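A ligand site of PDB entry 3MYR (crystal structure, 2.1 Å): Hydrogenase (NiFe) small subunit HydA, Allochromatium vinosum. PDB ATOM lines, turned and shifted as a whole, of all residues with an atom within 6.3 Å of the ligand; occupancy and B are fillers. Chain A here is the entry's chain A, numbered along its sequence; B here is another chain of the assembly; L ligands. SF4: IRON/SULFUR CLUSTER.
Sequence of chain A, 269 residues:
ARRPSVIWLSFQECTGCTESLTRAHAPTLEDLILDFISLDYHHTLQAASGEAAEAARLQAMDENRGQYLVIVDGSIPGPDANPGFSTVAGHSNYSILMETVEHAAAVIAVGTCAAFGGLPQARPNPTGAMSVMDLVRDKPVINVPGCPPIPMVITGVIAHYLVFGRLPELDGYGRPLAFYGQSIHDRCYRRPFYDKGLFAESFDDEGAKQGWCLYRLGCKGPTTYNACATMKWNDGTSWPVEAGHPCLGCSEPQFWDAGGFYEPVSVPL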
ATOM      1  N   GLN A  12     -13.096  22.315   3.923  1.00  0.00           N
ATOM      2  CA  GLN A  12     -12.301  22.368   2.677  1.00  0.00           C
ATOM      3  C   GLN A  12     -12.252  20.970   2.066  1.00  0.00           C
ATOM      4  O   GLN A  12     -11.184  20.263   2.105  1.00  0.00           O
ATOM      5  CB  GLN A  12     -10.875  22.869   2.919  1.00  0.00           C
ATOM      6  CG  GLN A  12     -10.821  24.309   3.489  1.00  0.00           C
ATOM      7  CD  GLN A  12      -9.375  24.658   3.715  1.00  0.00           C
ATOM      8  OE1 GLN A  12      -8.750  24.116   4.613  1.00  0.00           O
ATOM      9  NE2 GLN A  12      -8.815  25.587   2.903  1.00  0.00           N
ATOM     10  N   GLU A  13     -13.388  20.516   1.558  1.00  0.00           N
ATOM     11  CA  GLU A  13     -13.460  19.156   1.054  1.00  0.00           C
ATOM     12  C   GLU A  13     -13.669  19.191  -0.483  1.00  0.00           C
ATOM     13  O   GLU A  13     -14.052  20.256  -1.063  1.00  0.00           O
ATOM     14  CB  GLU A  13     -14.573  18.340   1.682  1.00  0.00           C
ATOM     15  CG  GLU A  13     -15.776  19.095   2.152  1.00  0.00           C
ATOM     16  CD  GLU A  13     -16.908  19.301   1.128  1.00  0.00           C
ATOM     17  OE1 GLU A  13     -17.252  20.515   0.814  1.00  0.00           O
ATOM     18  OE2 GLU A  13     -17.599  18.305   0.829  1.00  0.00           O
ATOM     19  N   CYS A  14     -13.574  18.009  -1.092  1.00  0.00           N
ATOM     20  CA  CYS A  14     -13.846  17.960  -2.525  1.00  0.00           C
ATOM     21  C   CYS A  14     -15.193  17.228  -2.750  1.00  0.00           C
ATOM     22  O   CYS A  14     -15.629  17.073  -3.882  1.00  0.00           O
ATOM     23  CB  CYS A  14     -12.635  17.218  -3.191  1.00  0.00           C
ATOM     24  SG  CYS A  14     -12.761  15.360  -3.077  1.00  0.00           S
ATOM     25  N   THR A  15     -15.788  16.742  -1.650  1.00  0.00           N
ATOM     26  CA  THR A  15     -17.097  16.048  -1.595  1.00  0.00           C
ATOM     27  C   THR A  15     -16.943  14.551  -1.970  1.00  0.00           C
ATOM     28  O   THR A  15     -17.896  13.780  -1.889  1.00  0.00           O
ATOM     29  CB  THR A  15     -18.274  16.814  -2.345  1.00  0.00           C
ATOM     30  OG1 THR A  15     -18.317  18.209  -1.907  1.00  0.00           O
ATOM     31  CG2 THR A  15     -19.708  16.163  -2.056  1.00  0.00           C
ATOM     32  N   GLY A  16     -15.733  14.121  -2.290  1.00  0.00           N
ATOM     33  CA  GLY A  16     -15.421  12.681  -2.380  1.00  0.00           C
ATOM     34  C   GLY A  16     -15.858  11.843  -1.201  1.00  0.00           C
ATOM     35  O   GLY A  16     -16.308  10.675  -1.393  1.00  0.00           O
ATOM     36  N   CYS A  17     -15.760  12.385   0.013  1.00  0.00           N
ATOM     37  CA  CYS A  17     -16.097  11.569   1.161  1.00  0.00           C
ATOM     38  C   CYS A  17     -17.585  11.354   1.259  1.00  0.00           C
ATOM     39  O   CYS A  17     -18.043  10.274   1.648  1.00  0.00           O
ATOM     40  CB  CYS A  17     -15.473  12.158   2.487  1.00  0.00           C
ATOM     41  SG  CYS A  17     -13.640  12.179   2.425  1.00  0.00           S
ATOM     42  N   ASP A  73     -15.898  16.575   7.155  1.00  0.00           N
ATOM     43  CA  ASP A  73     -15.316  16.283   5.859  1.00  0.00           C
ATOM     44  C   ASP A  73     -14.453  17.543   5.534  1.00  0.00           C
ATOM     45  O   ASP A  73     -14.983  18.653   5.528  1.00  0.00           O
ATOM     46  CB  ASP A  73     -16.499  16.218   4.836  1.00  0.00           C
ATOM     47  CG  ASP A  73     -16.064  15.611   3.590  1.00  0.00           C
ATOM     48  OD1 ASP A  73     -14.863  15.314   3.562  1.00  0.00           O
ATOM     49  OD2 ASP A  73     -16.841  15.472   2.620  1.00  0.00           O
ATOM     50  N   GLY A  74     -13.174  17.380   5.127  1.00  0.00           N
ATOM     51  CA  GLY A  74     -12.338  18.543   4.706  1.00  0.00           C
ATOM     52  C   GLY A  74     -11.494  19.095   5.849  1.00  0.00           C
ATOM     53  O   GLY A  74     -11.840  18.963   7.010  1.00  0.00           O
ATOM     54  N   SER A  75     -10.405  19.765   5.507  1.00  0.00           N
ATOM     55  CA  SER A  75      -9.560  20.471   6.456  1.00  0.00           C
ATOM     56  C   SER A  75     -10.204  21.813   6.794  1.00  0.00           C
ATOM     57  O   SER A  75     -11.206  22.191   6.208  1.00  0.00           O
ATOM     58  CB  SER A  75      -8.129  20.652   5.879  1.00  0.00           C
ATOM     59  OG  SER A  75      -8.275  21.420   4.673  1.00  0.00           O
ATOM     60  N   VAL A 110     -13.765  12.197   8.743  1.00  0.00           N
ATOM     61  CA  VAL A 110     -13.797  11.291   7.593  1.00  0.00           C
ATOM     62  C   VAL A 110     -12.910  11.867   6.500  1.00  0.00           C
ATOM     63  O   VAL A 110     -13.004  13.069   6.148  1.00  0.00           O
ATOM     64  CB  VAL A 110     -15.263  11.065   7.130  1.00  0.00           C
ATOM     65  CG1 VAL A 110     -15.792  12.390   6.560  1.00  0.00           C
ATOM     66  CG2 VAL A 110     -15.277  10.109   5.895  1.00  0.00           C
ATOM     67  N   GLY A 111     -12.018  11.039   5.950  1.00  0.00           N
ATOM     68  CA  GLY A 111     -11.146  11.508   4.855  1.00  0.00           C
ATOM     69  C   GLY A 111      -9.811  11.987   5.436  1.00  0.00           C
ATOM     70  O   GLY A 111      -9.732  12.500   6.576  1.00  0.00           O
ATOM     71  N   THR A 112      -8.761  11.821   4.658  1.00  0.00           N
ATOM     72  CA  THR A 112      -7.445  12.258   5.038  1.00  0.00           C
ATOM     73  C   THR A 112      -7.342  13.810   5.276  1.00  0.00           C
ATOM     74  O   THR A 112      -6.544  14.240   6.099  1.00  0.00           O
ATOM     75  CB  THR A 112      -6.405  11.797   3.969  1.00  0.00           C
ATOM     76  OG1 THR A 112      -6.463  10.379   3.891  1.00  0.00           O
ATOM     77  CG2 THR A 112      -4.932  12.198   4.349  1.00  0.00           C
ATOM     78  N   CYS A 113      -8.136  14.617   4.574  1.00  0.00           N
ATOM     79  CA  CYS A 113      -8.046  16.067   4.839  1.00  0.00           C
ATOM     80  C   CYS A 113      -8.492  16.419   6.262  1.00  0.00           C
ATOM     81  O   CYS A 113      -7.795  17.127   7.016  1.00  0.00           O
ATOM     82  CB  CYS A 113      -8.891  16.837   3.829  1.00  0.00           C
ATOM     83  SG  CYS A 113      -8.450  16.564   2.047  1.00  0.00           S
ATOM     84  N   ALA A 114      -9.661  15.939   6.660  1.00  0.00           N
ATOM     85  CA  ALA A 114     -10.141  16.203   8.021  1.00  0.00           C
ATOM     86  C   ALA A 114      -9.236  15.522   9.055  1.00  0.00           C
ATOM     87  O   ALA A 114      -8.956  16.093  10.097  1.00  0.00           O
ATOM     88  CB  ALA A 114     -11.584  15.723   8.171  1.00  0.00           C
ATOM     89  N   GLY A 118      -4.488  16.534   4.843  1.00  0.00           N
ATOM     90  CA  GLY A 118      -4.830  16.198   3.451  1.00  0.00           C
ATOM     91  C   GLY A 118      -4.319  17.240   2.398  1.00  0.00           C
ATOM     92  O   GLY A 118      -3.279  17.860   2.527  1.00  0.00           O
ATOM     93  N   LEU A 119      -5.085  17.396   1.331  1.00  0.00           N
ATOM     94  CA  LEU A 119      -4.618  18.111   0.188  1.00  0.00           C
ATOM     95  C   LEU A 119      -4.445  19.599   0.456  1.00  0.00           C
ATOM     96  O   LEU A 119      -3.434  20.146   0.096  1.00  0.00           O
ATOM     97  CB  LEU A 119      -5.577  17.894  -0.954  1.00  0.00           C
ATOM     98  CG  LEU A 119      -5.205  18.177  -2.374  1.00  0.00           C
ATOM     99  CD1 LEU A 119      -6.334  18.472  -3.350  1.00  0.00           C
ATOM    100  CD2 LEU A 119      -3.762  18.467  -2.727  1.00  0.00           C
ATOM    101  N   PRO A 120      -5.453  20.265   1.041  1.00  0.00           N
ATOM    102  CA  PRO A 120      -5.269  21.714   1.316  1.00  0.00           C
ATOM    103  C   PRO A 120      -4.011  22.005   2.179  1.00  0.00           C
ATOM    104  O   PRO A 120      -3.386  23.083   2.092  1.00  0.00           O
ATOM    105  CB  PRO A 120      -6.539  22.104   2.121  1.00  0.00           C
ATOM    106  CG  PRO A 120      -7.617  21.064   1.638  1.00  0.00           C
ATOM    107  CD  PRO A 120      -6.724  19.737   1.559  1.00  0.00           C
ATOM    108  N   GLY A 146      -8.142   8.142   4.199  1.00  0.00           N
ATOM    109  CA  GLY A 146      -8.399   7.630   2.836  1.00  0.00           C
ATOM    110  C   GLY A 146      -8.895   8.790   1.985  1.00  0.00           C
ATOM    111  O   GLY A 146      -9.458   9.716   2.510  1.00  0.00           O
ATOM    112  N   CYS A 147      -8.726   8.731   0.672  1.00  0.00           N
ATOM    113  CA  CYS A 147      -9.010   9.886  -0.166  1.00  0.00           C
ATOM    114  C   CYS A 147      -9.795   9.366  -1.397  1.00  0.00           C
ATOM    115  O   CYS A 147      -9.228   9.157  -2.491  1.00  0.00           O
ATOM    116  CB  CYS A 147      -7.659  10.536  -0.559  1.00  0.00           C
ATOM    117  SG  CYS A 147      -7.924  12.143  -1.322  1.00  0.00           S
ATOM    118  N   PRO A 148     -11.073   8.996  -1.187  1.00  0.00           N
ATOM    119  CA  PRO A 148     -11.782   9.023   0.112  1.00  0.00           C
ATOM    120  C   PRO A 148     -11.601   7.631   0.761  1.00  0.00           C
ATOM    121  O   PRO A 148     -11.003   6.735   0.142  1.00  0.00           O
ATOM    122  CB  PRO A 148     -13.238   9.261  -0.292  1.00  0.00           C
ATOM    123  CG  PRO A 148     -13.365   8.549  -1.689  1.00  0.00           C
ATOM    124  CD  PRO A 148     -11.949   8.602  -2.314  1.00  0.00           C
ATOM    125  N   PRO A 149     -12.025   7.465   2.011  1.00  0.00           N
ATOM    126  CA  PRO A 149     -12.061   6.162   2.659  1.00  0.00           C
ATOM    127  C   PRO A 149     -13.004   5.260   1.843  1.00  0.00           C
ATOM    128  O   PRO A 149     -13.932   5.729   1.173  1.00  0.00           O
ATOM    129  CB  PRO A 149     -12.749   6.473   4.057  1.00  0.00           C
ATOM    130  CG  PRO A 149     -12.527   8.034   4.245  1.00  0.00           C
ATOM    131  CD  PRO A 149     -12.707   8.510   2.814  1.00  0.00           C
ATOM    132  N   CYS A 250      -2.896   6.865   0.245  1.00  0.00           N
ATOM    133  CA  CYS A 250      -3.823   8.008   0.402  1.00  0.00           C
ATOM    134  C   CYS A 250      -4.505   8.097   1.789  1.00  0.00           C
ATOM    135  O   CYS A 250      -5.123   9.111   2.100  1.00  0.00           O
ATOM    136  CB  CYS A 250      -4.853   8.108  -0.715  1.00  0.00           C
ATOM    137  SG  CYS A 250      -6.198   6.863  -0.473  1.00  0.00           S
ATOM    138  N   TRP A 256       0.679  13.348   0.312  1.00  0.00           N
ATOM    139  CA  TRP A 256       0.937  14.162  -0.876  1.00  0.00           C
ATOM    140  C   TRP A 256       2.371  14.615  -0.957  1.00  0.00           C
ATOM    141  O   TRP A 256       2.849  14.936  -2.036  1.00  0.00           O
ATOM    142  CB  TRP A 256       0.091  15.445  -0.893  1.00  0.00           C
ATOM    143  CG  TRP A 256      -1.414  15.127  -0.892  1.00  0.00           C
ATOM    144  CD1 TRP A 256      -2.283  15.297   0.137  1.00  0.00           C
ATOM    145  CD2 TRP A 256      -2.191  14.695  -2.009  1.00  0.00           C
ATOM    146  NE1 TRP A 256      -3.561  14.889  -0.229  1.00  0.00           N
ATOM    147  CE2 TRP A 256      -3.539  14.570  -1.560  1.00  0.00           C
ATOM    148  CE3 TRP A 256      -1.879  14.383  -3.354  1.00  0.00           C
ATOM    149  CZ2 TRP A 256      -4.598  14.157  -2.403  1.00  0.00           C
ATOM    150  CZ3 TRP A 256      -2.896  13.957  -4.211  1.00  0.00           C
ATOM    151  CH2 TRP A 256      -4.263  13.784  -3.716  1.00  0.00           C
ATOM    152  N   ARG B  39      -8.859  26.441  -1.761  1.00  0.00           N
ATOM    153  CA  ARG B  39      -7.747  25.561  -1.341  1.00  0.00           C
ATOM    154  C   ARG B  39      -6.374  25.921  -1.970  1.00  0.00           C
ATOM    155  O   ARG B  39      -5.318  25.731  -1.341  1.00  0.00           O
ATOM    156  CB  ARG B  39      -8.063  24.076  -1.560  1.00  0.00           C
ATOM    157  CG  ARG B  39      -9.218  23.609  -0.676  1.00  0.00           C
ATOM    158  CD  ARG B  39      -9.902  22.316  -1.116  1.00  0.00           C
ATOM    159  NE  ARG B  39     -10.496  22.490  -2.445  1.00  0.00           N
ATOM    160  CZ  ARG B  39     -10.803  21.495  -3.272  1.00  0.00           C
ATOM    161  NH1 ARG B  39     -10.527  20.229  -2.939  1.00  0.00           N
ATOM    162  NH2 ARG B  39     -11.289  21.797  -4.486  1.00  0.00           N
ATOM    163  N   ARG B  59      -8.516  15.488  -7.013  1.00  0.00           N
ATOM    164  CA  ARG B  59      -9.065  15.892  -5.703  1.00  0.00           C
ATOM    165  C   ARG B  59      -9.530  17.353  -5.675  1.00  0.00           C
ATOM    166  O   ARG B  59      -9.995  17.817  -4.646  1.00  0.00           O
ATOM    167  CB  ARG B  59      -8.064  15.596  -4.556  1.00  0.00           C
ATOM    168  CG  ARG B  59      -8.205  14.139  -4.033  1.00  0.00           C
ATOM    169  CD  ARG B  59      -7.846  13.055  -5.117  1.00  0.00           C
ATOM    170  NE  ARG B  59      -7.632  11.759  -4.474  1.00  0.00           N
ATOM    171  CZ  ARG B  59      -7.116  10.701  -5.088  1.00  0.00           C
ATOM    172  NH1 ARG B  59      -6.564  10.842  -6.296  1.00  0.00           N
ATOM    173  NH2 ARG B  59      -7.119   9.489  -4.471  1.00  0.00           N
ATOM    174  N   GLY B  62     -14.724  15.517  -5.948  1.00  0.00           N
ATOM    175  CA  GLY B  62     -15.110  14.133  -5.967  1.00  0.00           C
ATOM    176  C   GLY B  62     -16.523  13.868  -6.475  1.00  0.00           C
ATOM    177  O   GLY B  62     -16.975  12.713  -6.497  1.00  0.00           O
ATOM    178  N   PRO B 213     -15.319   6.827  -5.319  1.00  0.00           N
ATOM    179  CA  PRO B 213     -14.691   7.923  -6.092  1.00  0.00           C
ATOM    180  C   PRO B 213     -13.152   7.840  -6.288  1.00  0.00           C
ATOM    181  O   PRO B 213     -12.446   7.078  -5.591  1.00  0.00           O
ATOM    182  CB  PRO B 213     -15.040   9.191  -5.257  1.00  0.00           C
ATOM    183  CG  PRO B 213     -16.322   8.752  -4.388  1.00  0.00           C
ATOM    184  CD  PRO B 213     -15.913   7.326  -4.052  1.00  0.00           C
ATOM    185  N   HIS B 214     -12.670   8.700  -7.185  1.00  0.00           N
ATOM    186  CA  HIS B 214     -11.286   8.915  -7.436  1.00  0.00           C
ATOM    187  C   HIS B 214     -10.526   7.741  -8.054  1.00  0.00           C
ATOM    188  O   HIS B 214      -9.496   7.304  -7.524  1.00  0.00           O
ATOM    189  CB  HIS B 214     -10.641   9.540  -6.161  1.00  0.00           C
ATOM    190  CG  HIS B 214     -11.080  10.960  -5.933  1.00  0.00           C
ATOM    191  ND1 HIS B 214     -11.041  11.590  -4.711  1.00  0.00           N
ATOM    192  CD2 HIS B 214     -11.660  11.830  -6.785  1.00  0.00           C
ATOM    193  CE1 HIS B 214     -11.542  12.812  -4.825  1.00  0.00           C
ATOM    194  NE2 HIS B 214     -11.891  12.987  -6.086  1.00  0.00           N
HETATM  195 FE1  SF4 L   1      -9.779  13.149  -0.496  1.00  0.00          FE
HETATM  196 FE2  SF4 L   1     -12.068  13.220   1.095  1.00  0.00          FE
HETATM  197 FE3  SF4 L   1     -10.082  15.223   1.312  1.00  0.00          FE
HETATM  198 FE4  SF4 L   1     -11.879  14.759  -1.035  1.00  0.00          FE
HETATM  199  S1  SF4 L   1     -12.409  15.570   1.193  1.00  0.00           S
HETATM  200  S2  SF4 L   1      -9.731  15.388  -0.906  1.00  0.00           S
HETATM  201  S3  SF4 L   1     -11.797  12.481  -1.099  1.00  0.00           S
HETATM  202  S4  SF4 L   1      -9.829  13.018   1.760  1.00  0.00           S
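The backbone NH (N) of Cys 113 sits close to a sulfur (S4) of the ligand (3.7 Å).
SG of Cys 113 binds FE3 of the ligand, 2.2 Å away.
The side-chain sulfur (SG) of Cys 147 is bound to an iron atom (FE1) of the ligand (2.3 Å).
The backbone NH (N) of Cys 14 sits close to a sulfur (S1) of the ligand (3.5 Å).
An iron atom (FE4) of the ligand is bound by the side-chain sulfur of Cys 14, at 2.3 Å.
SG of Cys 17 binds FE2 of the ligand (2.3 Å).
A sulfur (S4) of the ligand sits close to the backbone NH (N) of Thr 112 (3.3 Å).
ND1 of His 214 of chain B sits close to S3 of the ligand (3.8 Å).
The side-chain sulfur of Cys 113 sits close to the backbone NH of Leu 119.
The guanidinium group (NH2) of Arg 59 of chain B lies within hydrogen-bond range of the backbone carbonyl oxygen (O) of Cys 147.
The backbone NH of Cys 147 sits close to the side-chain sulfur of Cys 250 (3.3 Å).
N of Gly 16 sits close to SG of Cys 14 (3.3 Å).
SG of Cys 17 sits close to OD1 of Asp 73.
OG1 of Thr 112 is in hydrogen-bond range of N of Gly 146.
O of Thr 112 sits at hydrogen-bond distance from N of Gly 118 (3.3 Å).
The side-chain hydroxyl (OG1) of Thr 112 is in hydrogen-bond range of the backbone carbonyl oxygen (O) of Cys 250 (2.6 Å).
The side-chain carboxylate (OD1) of Asp 73 sits close to a sulfur (S1) of the ligand (3.4 Å).
O of Gly 146 sits close to S4 of the ligand, at 3.4 Å.
The backbone nitrogen (N) of Pro 148 lies close to a sulfur (S3) of the ligand.
Glu 13 touches the ligand.
Gly 16 touches the ligand.
Gly 111 touches the ligand (CA to S4, 3.7 Å).
CG of Arg 59 of chain B touches S2 of the ligand, 3.7 Å away.
Hydrophobic or aromatic side chains within 4 Å of the ligand: Pro 148 and His 214 of chain B.
Within 4 Å of the ligand: Glu 13, Cys 14, Gly 16, Cys 17, Asp 73, Gly 111, Thr 112, Cys 113, Gly 146, Cys 147, Pro 148, Arg 59 of chain B and His 214 of chain B.
The nearest printed residue that does not touch the ligand is Gly 74 (4.4 Å).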
